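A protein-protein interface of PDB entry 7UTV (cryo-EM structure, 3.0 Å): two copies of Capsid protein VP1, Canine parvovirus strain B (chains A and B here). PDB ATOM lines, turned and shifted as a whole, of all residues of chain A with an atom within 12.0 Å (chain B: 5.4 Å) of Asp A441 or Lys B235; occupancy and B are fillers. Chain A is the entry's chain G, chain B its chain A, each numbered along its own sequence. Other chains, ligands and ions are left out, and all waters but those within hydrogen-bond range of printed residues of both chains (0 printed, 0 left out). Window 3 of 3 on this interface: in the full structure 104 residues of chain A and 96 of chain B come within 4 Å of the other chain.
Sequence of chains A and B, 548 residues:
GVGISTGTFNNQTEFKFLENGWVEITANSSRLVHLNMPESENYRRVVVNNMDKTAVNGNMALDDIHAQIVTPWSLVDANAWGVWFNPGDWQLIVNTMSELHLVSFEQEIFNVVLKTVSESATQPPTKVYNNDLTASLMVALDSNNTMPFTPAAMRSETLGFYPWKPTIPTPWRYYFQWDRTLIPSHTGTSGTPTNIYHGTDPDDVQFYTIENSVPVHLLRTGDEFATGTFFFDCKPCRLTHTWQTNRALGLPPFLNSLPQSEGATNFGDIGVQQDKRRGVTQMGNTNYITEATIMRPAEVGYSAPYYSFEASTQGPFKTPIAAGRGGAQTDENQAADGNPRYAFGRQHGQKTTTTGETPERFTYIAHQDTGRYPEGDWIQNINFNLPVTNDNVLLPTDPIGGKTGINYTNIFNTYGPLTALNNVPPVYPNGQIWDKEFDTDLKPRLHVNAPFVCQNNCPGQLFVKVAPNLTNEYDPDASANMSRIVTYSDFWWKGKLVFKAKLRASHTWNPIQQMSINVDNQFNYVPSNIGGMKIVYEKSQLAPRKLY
Thr A440 touches Leu B421 (CB to O, 3.4 Å).
Thr A440 touches Asn B422 (CG2 to OD1, 3.4 Å).
CA of Thr A440 touches NH2 of Arg B545, at 3.5 Å.
Lys B235 touches Asp A441.
OD1 of Asp A441 touches CD of Arg B238 (3.5 Å).
CA of Asn B422 touches OD2 of Asp A441, 3.5 Å away.
Arg B545 touches Asp A441.
The side-chain amide oxygen of Asn B422 lies within hydrogen-bond range of the guanidinium group of Arg B545 (2.9 Å).
The side-chain hydroxyl (OG1) of Thr A440 sits at hydrogen-bond distance from the backbone carbonyl oxygen (O) of Leu A442, at 3.3 Å.
The backbone carbonyl oxygen (O) of Thr A440 sits at hydrogen-bond distance from the side-chain amino group (NZ) of Lys A443 (2.9 Å).
1 position is printed for both chains.
Of the printed residues of chain B, Asp A439 touches Arg B238 (2.9 Å) and Arg B545 (2.6 Å).
Printed residues of chain B within 4 Å of Thr A440: Leu B421 (3.4 Å), Asn B422 (3.4 Å) and Arg B545 (3.5 Å).
Of the printed residues of chain B, Asp A441 touches Lys B235, Arg B238, Leu B421, Asn B422, Asn B423 and Arg B545.
Printed residues of chain B within 4 Å of Leu A442: Leu B421 (2.8 Å).
Pro A444 touches none of the printed residues of chain B.
No residue of chain A comes within 4 Å of His B101.
No residue of chain A comes within 4 Å of Asp B233.
No residue of chain A comes within 4 Å of Cys B234.
Lys B235 touches just one residue of chain A: Asp A441.
No residue of chain A comes within 4 Å of Pro B236.
Printed residues of chain A within 4 Å of Arg B238: Asp A439 and Asp A441.
Printed residues of chain A within 4 Å of Leu B421: Thr A440, Asp A441 and Leu A442.
Of chain A, only Thr A440 (3.4 Å) and Asp A441 (3.5 Å) come within 4 Å of Asn B422.
Of chain A, only Asp A441 (2.6 Å) comes within 4 Å of Asn B423.
Of the printed residues of chain A, Arg B545 touches Asp A439 (2.6 Å), Thr A440 (3.5 Å) and Asp A441 (3.99 Å).
The nearest printed residue of chain B that does not touch Asp A441 is Pro B236 (4.6 Å).
The nearest residue of chain A that does not touch Lys B235 is Leu A442 (4.8 Å).
The side-chain carboxylate (OD1) of Asp A439 lies within salt-bridge range of the guanidinium group (NH1) of Arg B238 (2.9 Å).
The backbone NH (N) of Asp A441 is in hydrogen-bond range of the backbone carbonyl oxygen (O) of Leu B421 (3.4 Å).
N of Leu A442 lies within hydrogen-bond range of O of Leu B421 (2.8 Å).
The side-chain carboxylate of Asp A441 lies within hydrogen-bond range of the backbone NH of Asn B423 (2.6 Å).
The guanidinium group (NE) of Arg B545 lies within salt-bridge range of the side-chain carboxylate (OD2) of Asp A439.
Of the 12 printed residues of chain A, 4 touch a printed residue of chain B.
Among the printed residues, Asp or Glu carboxylates within 4 Å of a Lys or Arg side-chain nitrogen of the other chain: Asp A439 with Arg B238 (2.9 Å) and Asp A439 with Arg B545 (2.6 Å).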
ATOM      1  N   LYS A 436      27.147 -25.400  11.905  1.00  0.00           N
ATOM      2  CA  LYS A 436      26.068 -24.883  11.081  1.00  0.00           C
ATOM      3  C   LYS A 436      26.352 -25.174   9.617  1.00  0.00           C
ATOM      4  O   LYS A 436      27.481 -25.007   9.149  1.00  0.00           O
ATOM      5  CB  LYS A 436      25.899 -23.386  11.302  1.00  0.00           C
ATOM      6  CG  LYS A 436      24.576 -22.858  10.797  1.00  0.00           C
ATOM      7  CD  LYS A 436      24.512 -21.347  10.847  1.00  0.00           C
ATOM      8  CE  LYS A 436      25.169 -20.702   9.637  1.00  0.00           C
ATOM      9  NZ  LYS A 436      24.444 -20.980   8.363  1.00  0.00           N
ATOM     10  N   GLU A 437      25.328 -25.610   8.895  1.00  0.00           N
ATOM     11  CA  GLU A 437      25.475 -25.843   7.469  1.00  0.00           C
ATOM     12  C   GLU A 437      25.632 -24.519   6.735  1.00  0.00           C
ATOM     13  O   GLU A 437      25.138 -23.478   7.169  1.00  0.00           O
ATOM     14  CB  GLU A 437      24.268 -26.616   6.940  1.00  0.00           C
ATOM     15  CG  GLU A 437      24.310 -27.011   5.465  1.00  0.00           C
ATOM     16  CD  GLU A 437      25.458 -27.943   5.131  1.00  0.00           C
ATOM     17  OE1 GLU A 437      26.612 -27.471   5.064  1.00  0.00           O
ATOM     18  OE2 GLU A 437      25.204 -29.150   4.939  1.00  0.00           O
ATOM     19  N   PHE A 438      26.340 -24.568   5.616  1.00  0.00           N
ATOM     20  CA  PHE A 438      26.567 -23.375   4.819  1.00  0.00           C
ATOM     21  C   PHE A 438      25.270 -22.918   4.167  1.00  0.00           C
ATOM     22  O   PHE A 438      24.386 -23.721   3.865  1.00  0.00           O
ATOM     23  CB  PHE A 438      27.620 -23.643   3.738  1.00  0.00           C
ATOM     24  CG  PHE A 438      29.060 -23.714   4.234  1.00  0.00           C
ATOM     25  CD1 PHE A 438      29.390 -23.771   5.572  1.00  0.00           C
ATOM     26  CD2 PHE A 438      30.089 -23.720   3.314  1.00  0.00           C
ATOM     27  CE1 PHE A 438      30.691 -23.833   5.972  1.00  0.00           C
ATOM     28  CE2 PHE A 438      31.398 -23.779   3.715  1.00  0.00           C
ATOM     29  CZ  PHE A 438      31.699 -23.836   5.048  1.00  0.00           C
ATOM     30  N   ASP A 439      25.157 -21.611   3.972  1.00  0.00           N
ATOM     31  CA  ASP A 439      24.036 -20.982   3.288  1.00  0.00           C
ATOM     32  C   ASP A 439      24.105 -21.120   1.770  1.00  0.00           C
ATOM     33  O   ASP A 439      23.207 -20.621   1.088  1.00  0.00           O
ATOM     34  CB  ASP A 439      24.002 -19.503   3.681  1.00  0.00           C
ATOM     35  CG  ASP A 439      22.658 -18.853   3.428  1.00  0.00           C
ATOM     36  OD1 ASP A 439      21.637 -19.380   3.921  1.00  0.00           O
ATOM     37  OD2 ASP A 439      22.619 -17.812   2.737  1.00  0.00           O
ATOM     38  N   THR A 440      25.132 -21.773   1.230  1.00  0.00           N
ATOM     39  CA  THR A 440      25.287 -21.902  -0.210  1.00  0.00           C
ATOM     40  C   THR A 440      24.140 -22.693  -0.814  1.00  0.00           C
ATOM     41  O   THR A 440      23.451 -23.453  -0.133  1.00  0.00           O
ATOM     42  CB  THR A 440      26.602 -22.600  -0.538  1.00  0.00           C
ATOM     43  OG1 THR A 440      26.974 -23.459   0.548  1.00  0.00           O
ATOM     44  CG2 THR A 440      27.705 -21.597  -0.794  1.00  0.00           C
ATOM     45  N   ASP A 441      23.923 -22.488  -2.110  1.00  0.00           N
ATOM     46  CA  ASP A 441      22.914 -23.274  -2.802  1.00  0.00           C
ATOM     47  C   ASP A 441      23.329 -24.734  -2.879  1.00  0.00           C
ATOM     48  O   ASP A 441      22.522 -25.626  -2.597  1.00  0.00           O
ATOM     49  CB  ASP A 441      22.673 -22.703  -4.200  1.00  0.00           C
ATOM     50  CG  ASP A 441      22.237 -21.248  -4.168  1.00  0.00           C
ATOM     51  OD1 ASP A 441      21.332 -20.913  -3.374  1.00  0.00           O
ATOM     52  OD2 ASP A 441      22.801 -20.438  -4.935  1.00  0.00           O
ATOM     53  N   LEU A 442      24.583 -24.993  -3.237  1.00  0.00           N
ATOM     54  CA  LEU A 442      25.159 -26.328  -3.251  1.00  0.00           C
ATOM     55  C   LEU A 442      26.009 -26.490  -2.003  1.00  0.00           C
ATOM     56  O   LEU A 442      26.986 -25.757  -1.817  1.00  0.00           O
ATOM     57  CB  LEU A 442      26.014 -26.546  -4.493  1.00  0.00           C
ATOM     58  CG  LEU A 442      25.363 -26.344  -5.860  1.00  0.00           C
ATOM     59  CD1 LEU A 442      26.389 -26.603  -6.946  1.00  0.00           C
ATOM     60  CD2 LEU A 442      24.149 -27.237  -6.036  1.00  0.00           C
ATOM     61  N   LYS A 443      25.655 -27.452  -1.176  1.00  0.00           N
ATOM     62  CA  LYS A 443      26.150 -27.561   0.180  1.00  0.00           C
ATOM     63  C   LYS A 443      27.193 -28.663   0.273  1.00  0.00           C
ATOM     64  O   LYS A 443      27.065 -29.670  -0.429  1.00  0.00           O
ATOM     65  CB  LYS A 443      24.996 -27.857   1.138  1.00  0.00           C
ATOM     66  CG  LYS A 443      23.912 -26.796   1.111  1.00  0.00           C
ATOM     67  CD  LYS A 443      22.763 -27.111   2.032  1.00  0.00           C
ATOM     68  CE  LYS A 443      21.546 -26.253   1.714  1.00  0.00           C
ATOM     69  NZ  LYS A 443      21.783 -24.791   1.889  1.00  0.00           N
ATOM     70  N   PRO A 444      28.243 -28.515   1.087  1.00  0.00           N
ATOM     71  CA  PRO A 444      29.269 -29.555   1.129  1.00  0.00           C
ATOM     72  C   PRO A 444      28.723 -30.843   1.711  1.00  0.00           C
ATOM     73  O   PRO A 444      27.831 -30.839   2.559  1.00  0.00           O
ATOM     74  CB  PRO A 444      30.348 -28.948   2.021  1.00  0.00           C
ATOM     75  CG  PRO A 444      29.635 -28.075   2.894  1.00  0.00           C
ATOM     76  CD  PRO A 444      28.508 -27.499   2.117  1.00  0.00           C
ATOM     77  N   ARG A 445      29.269 -31.961   1.237  1.00  0.00           N
ATOM     78  CA  ARG A 445      28.748 -33.256   1.648  1.00  0.00           C
ATOM     79  C   ARG A 445      29.081 -33.577   3.094  1.00  0.00           C
ATOM     80  O   ARG A 445      28.294 -34.251   3.765  1.00  0.00           O
ATOM     81  CB  ARG A 445      29.277 -34.350   0.732  1.00  0.00           C
ATOM     82  CG  ARG A 445      28.690 -34.298  -0.667  1.00  0.00           C
ATOM     83  CD  ARG A 445      28.306 -35.653  -1.201  1.00  0.00           C
ATOM     84  NE  ARG A 445      29.472 -36.424  -1.602  1.00  0.00           N
ATOM     85  CZ  ARG A 445      29.455 -37.702  -1.955  1.00  0.00           C
ATOM     86  NH1 ARG A 445      28.342 -38.422  -1.931  1.00  0.00           N
ATOM     87  NH2 ARG A 445      30.587 -38.277  -2.346  1.00  0.00           N
ATOM     88  N   HIS A 447      31.440 -31.896   6.742  1.00  0.00           N
ATOM     89  CA  HIS A 447      32.286 -30.896   7.370  1.00  0.00           C
ATOM     90  C   HIS A 447      33.435 -31.605   8.065  1.00  0.00           C
ATOM     91  O   HIS A 447      33.233 -32.617   8.741  1.00  0.00           O
ATOM     92  CB  HIS A 447      31.493 -30.064   8.376  1.00  0.00           C
ATOM     93  CG  HIS A 447      30.537 -29.104   7.746  1.00  0.00           C
ATOM     94  ND1 HIS A 447      30.184 -27.917   8.345  1.00  0.00           N
ATOM     95  CD2 HIS A 447      29.862 -29.149   6.575  1.00  0.00           C
ATOM     96  CE1 HIS A 447      29.330 -27.271   7.572  1.00  0.00           C
ATOM     97  NE2 HIS A 447      29.120 -27.997   6.490  1.00  0.00           N
ATOM     98  N   GLN A 455      21.360 -28.909   9.699  1.00  0.00           N
ATOM     99  CA  GLN A 455      20.994 -28.684   8.309  1.00  0.00           C
ATOM    100  C   GLN A 455      20.139 -27.434   8.128  1.00  0.00           C
ATOM    101  O   GLN A 455      20.398 -26.654   7.204  1.00  0.00           O
ATOM    102  CB  GLN A 455      20.281 -29.917   7.753  1.00  0.00           C
ATOM    103  CG  GLN A 455      21.143 -31.201   7.702  1.00  0.00           C
ATOM    104  CD  GLN A 455      22.481 -31.055   6.967  1.00  0.00           C
ATOM    105  OE1 GLN A 455      23.485 -31.631   7.385  1.00  0.00           O
ATOM    106  NE2 GLN A 455      22.498 -30.291   5.874  1.00  0.00           N
ATOM    107  N   LEU B 100      13.817 -15.535  -4.995  1.00  0.00           N
ATOM    108  CA  LEU B 100      12.907 -15.478  -6.118  1.00  0.00           C
ATOM    109  C   LEU B 100      12.589 -16.903  -6.539  1.00  0.00           C
ATOM    110  O   LEU B 100      13.497 -17.725  -6.679  1.00  0.00           O
ATOM    111  CB  LEU B 100      13.557 -14.686  -7.255  1.00  0.00           C
ATOM    112  CG  LEU B 100      12.801 -14.371  -8.537  1.00  0.00           C
ATOM    113  CD1 LEU B 100      11.564 -13.556  -8.273  1.00  0.00           C
ATOM    114  CD2 LEU B 100      13.721 -13.636  -9.485  1.00  0.00           C
ATOM    115  N   HIS B 101      11.302 -17.192  -6.731  1.00  0.00           N
ATOM    116  CA  HIS B 101      10.809 -18.486  -7.186  1.00  0.00           C
ATOM    117  C   HIS B 101      10.065 -18.266  -8.488  1.00  0.00           C
ATOM    118  O   HIS B 101       9.450 -17.216  -8.678  1.00  0.00           O
ATOM    119  CB  HIS B 101       9.825 -19.144  -6.209  1.00  0.00           C
ATOM    120  CG  HIS B 101      10.357 -19.368  -4.832  1.00  0.00           C
ATOM    121  ND1 HIS B 101      10.382 -20.615  -4.246  1.00  0.00           N
ATOM    122  CD2 HIS B 101      10.825 -18.507  -3.903  1.00  0.00           C
ATOM    123  CE1 HIS B 101      10.874 -20.514  -3.026  1.00  0.00           C
ATOM    124  NE2 HIS B 101      11.151 -19.244  -2.793  1.00  0.00           N
ATOM    125  N   ASP B 233       8.370 -26.112 -10.339  1.00  0.00           N
ATOM    126  CA  ASP B 233       8.622 -26.581  -8.984  1.00  0.00           C
ATOM    127  C   ASP B 233      10.059 -26.309  -8.568  1.00  0.00           C
ATOM    128  O   ASP B 233      10.601 -27.025  -7.721  1.00  0.00           O
ATOM    129  CB  ASP B 233       8.307 -28.071  -8.866  1.00  0.00           C
ATOM    130  CG  ASP B 233       9.188 -28.922  -9.754  1.00  0.00           C
ATOM    131  OD1 ASP B 233       9.706 -28.390 -10.759  1.00  0.00           O
ATOM    132  OD2 ASP B 233       9.366 -30.120  -9.449  1.00  0.00           O
ATOM    133  N   CYS B 234      10.690 -25.298  -9.157  1.00  0.00           N
ATOM    134  CA  CYS B 234      12.127 -25.113  -9.018  1.00  0.00           C
ATOM    135  C   CYS B 234      12.491 -24.568  -7.643  1.00  0.00           C
ATOM    136  O   CYS B 234      11.693 -23.914  -6.970  1.00  0.00           O
ATOM    137  CB  CYS B 234      12.652 -24.175 -10.106  1.00  0.00           C
ATOM    138  SG  CYS B 234      12.229 -24.685 -11.782  1.00  0.00           S
ATOM    139  N   LYS B 235      13.718 -24.865  -7.233  1.00  0.00           N
ATOM    140  CA  LYS B 235      14.243 -24.366  -5.980  1.00  0.00           C
ATOM    141  C   LYS B 235      14.547 -22.867  -6.095  1.00  0.00           C
ATOM    142  O   LYS B 235      14.732 -22.355  -7.200  1.00  0.00           O
ATOM    143  CB  LYS B 235      15.497 -25.149  -5.601  1.00  0.00           C
ATOM    144  CG  LYS B 235      16.683 -24.997  -6.552  1.00  0.00           C
ATOM    145  CD  LYS B 235      17.757 -26.051  -6.275  1.00  0.00           C
ATOM    146  CE  LYS B 235      18.506 -25.770  -4.984  1.00  0.00           C
ATOM    147  NZ  LYS B 235      19.566 -26.779  -4.741  1.00  0.00           N
ATOM    148  N   PRO B 236      14.581 -22.135  -4.977  1.00  0.00           N
ATOM    149  CA  PRO B 236      14.732 -20.676  -5.064  1.00  0.00           C
ATOM    150  C   PRO B 236      16.086 -20.232  -5.592  1.00  0.00           C
ATOM    151  O   PRO B 236      17.130 -20.732  -5.174  1.00  0.00           O
ATOM    152  CB  PRO B 236      14.537 -20.217  -3.618  1.00  0.00           C
ATOM    153  CG  PRO B 236      14.818 -21.382  -2.815  1.00  0.00           C
ATOM    154  CD  PRO B 236      14.332 -22.538  -3.584  1.00  0.00           C
ATOM    155  N   CYS B 237      16.053 -19.267  -6.504  1.00  0.00           N
ATOM    156  CA  CYS B 237      17.219 -18.456  -6.799  1.00  0.00           C
ATOM    157  C   CYS B 237      17.308 -17.364  -5.751  1.00  0.00           C
ATOM    158  O   CYS B 237      16.299 -16.755  -5.392  1.00  0.00           O
ATOM    159  CB  CYS B 237      17.122 -17.840  -8.195  1.00  0.00           C
ATOM    160  SG  CYS B 237      18.540 -16.830  -8.664  1.00  0.00           S
ATOM    161  N   ARG B 238      18.515 -17.120  -5.265  1.00  0.00           N
ATOM    162  CA  ARG B 238      18.756 -16.193  -4.171  1.00  0.00           C
ATOM    163  C   ARG B 238      19.452 -14.972  -4.740  1.00  0.00           C
ATOM    164  O   ARG B 238      20.500 -15.095  -5.381  1.00  0.00           O
ATOM    165  CB  ARG B 238      19.583 -16.859  -3.077  1.00  0.00           C
ATOM    166  CG  ARG B 238      18.871 -18.047  -2.480  1.00  0.00           C
ATOM    167  CD  ARG B 238      19.608 -18.645  -1.322  1.00  0.00           C
ATOM    168  NE  ARG B 238      19.546 -17.781  -0.153  1.00  0.00           N
ATOM    169  CZ  ARG B 238      19.881 -18.138   1.080  1.00  0.00           C
ATOM    170  NH1 ARG B 238      20.254 -19.378   1.374  1.00  0.00           N
ATOM    171  NH2 ARG B 238      19.838 -17.229   2.049  1.00  0.00           N
ATOM    172  N   LEU B 421      29.226 -24.213  -3.260  1.00  0.00           N
ATOM    173  CA  LEU B 421      29.070 -23.333  -4.402  1.00  0.00           C
ATOM    174  C   LEU B 421      27.682 -22.725  -4.395  1.00  0.00           C
ATOM    175  O   LEU B 421      26.741 -23.302  -3.849  1.00  0.00           O
ATOM    176  CB  LEU B 421      29.285 -24.090  -5.706  1.00  0.00           C
ATOM    177  CG  LEU B 421      30.729 -24.396  -6.077  1.00  0.00           C
ATOM    178  CD1 LEU B 421      30.751 -25.515  -7.058  1.00  0.00           C
ATOM    179  CD2 LEU B 421      31.437 -23.171  -6.643  1.00  0.00           C
ATOM    180  N   ASN B 422      27.569 -21.558  -5.013  1.00  0.00           N
ATOM    181  CA  ASN B 422      26.295 -20.906  -5.258  1.00  0.00           C
ATOM    182  C   ASN B 422      25.805 -21.197  -6.670  1.00  0.00           C
ATOM    183  O   ASN B 422      26.579 -21.535  -7.567  1.00  0.00           O
ATOM    184  CB  ASN B 422      26.434 -19.404  -5.068  1.00  0.00           C
ATOM    185  CG  ASN B 422      26.657 -19.022  -3.634  1.00  0.00           C
ATOM    186  OD1 ASN B 422      25.958 -19.498  -2.744  1.00  0.00           O
ATOM    187  ND2 ASN B 422      27.626 -18.149  -3.392  1.00  0.00           N
ATOM    188  N   ASN B 423      24.501 -21.055  -6.864  1.00  0.00           N
ATOM    189  CA  ASN B 423      23.958 -21.095  -8.207  1.00  0.00           C
ATOM    190  C   ASN B 423      24.391 -19.847  -8.966  1.00  0.00           C
ATOM    191  O   ASN B 423      24.778 -18.838  -8.375  1.00  0.00           O
ATOM    192  CB  ASN B 423      22.437 -21.202  -8.161  1.00  0.00           C
ATOM    193  CG  ASN B 423      21.852 -21.796  -9.419  1.00  0.00           C
ATOM    194  OD1 ASN B 423      22.525 -21.907 -10.443  1.00  0.00           O
ATOM    195  ND2 ASN B 423      20.583 -22.182  -9.352  1.00  0.00           N
ATOM    196  N   PHE B 452      17.244 -21.231 -12.482  1.00  0.00           N
ATOM    197  CA  PHE B 452      16.253 -22.271 -12.253  1.00  0.00           C
ATOM    198  C   PHE B 452      16.432 -23.395 -13.255  1.00  0.00           C
ATOM    199  O   PHE B 452      16.772 -23.156 -14.417  1.00  0.00           O
ATOM    200  CB  PHE B 452      14.846 -21.695 -12.363  1.00  0.00           C
ATOM    201  CG  PHE B 452      14.624 -20.500 -11.498  1.00  0.00           C
ATOM    202  CD1 PHE B 452      14.414 -20.639 -10.153  1.00  0.00           C
ATOM    203  CD2 PHE B 452      14.622 -19.241 -12.037  1.00  0.00           C
ATOM    204  CE1 PHE B 452      14.211 -19.547  -9.364  1.00  0.00           C
ATOM    205  CE2 PHE B 452      14.422 -18.143 -11.255  1.00  0.00           C
ATOM    206  CZ  PHE B 452      14.216 -18.294  -9.914  1.00  0.00           C
ATOM    207  N   GLN B 455      12.933 -29.718 -12.853  1.00  0.00           N
ATOM    208  CA  GLN B 455      13.318 -31.018 -12.322  1.00  0.00           C
ATOM    209  C   GLN B 455      12.800 -32.178 -13.167  1.00  0.00           C
ATOM    210  O   GLN B 455      13.573 -33.099 -13.450  1.00  0.00           O
ATOM    211  CB  GLN B 455      12.839 -31.147 -10.876  1.00  0.00           C
ATOM    212  CG  GLN B 455      13.562 -30.229  -9.870  1.00  0.00           C
ATOM    213  CD  GLN B 455      15.079 -30.424  -9.808  1.00  0.00           C
ATOM    214  OE1 GLN B 455      15.825 -29.451  -9.701  1.00  0.00           O
ATOM    215  NE2 GLN B 455      15.537 -31.672  -9.882  1.00  0.00           N
ATOM    216  N   ARG B 545      25.042 -11.582   1.834  1.00  0.00           N
ATOM    217  CA  ARG B 545      24.411 -12.531   2.745  1.00  0.00           C
ATOM    218  C   ARG B 545      25.472 -13.313   3.497  1.00  0.00           C
ATOM    219  O   ARG B 545      26.621 -13.430   3.066  1.00  0.00           O
ATOM    220  CB  ARG B 545      23.451 -13.496   2.025  1.00  0.00           C
ATOM    221  CG  ARG B 545      24.013 -14.803   1.496  1.00  0.00           C
ATOM    222  CD  ARG B 545      22.963 -15.497   0.676  1.00  0.00           C
ATOM    223  NE  ARG B 545      23.281 -16.891   0.388  1.00  0.00           N
ATOM    224  CZ  ARG B 545      23.721 -17.386  -0.765  1.00  0.00           C
ATOM    225  NH1 ARG B 545      23.981 -16.619  -1.817  1.00  0.00           N
ATOM    226  NH2 ARG B 545      23.915 -18.696  -0.869  1.00  0.00           N
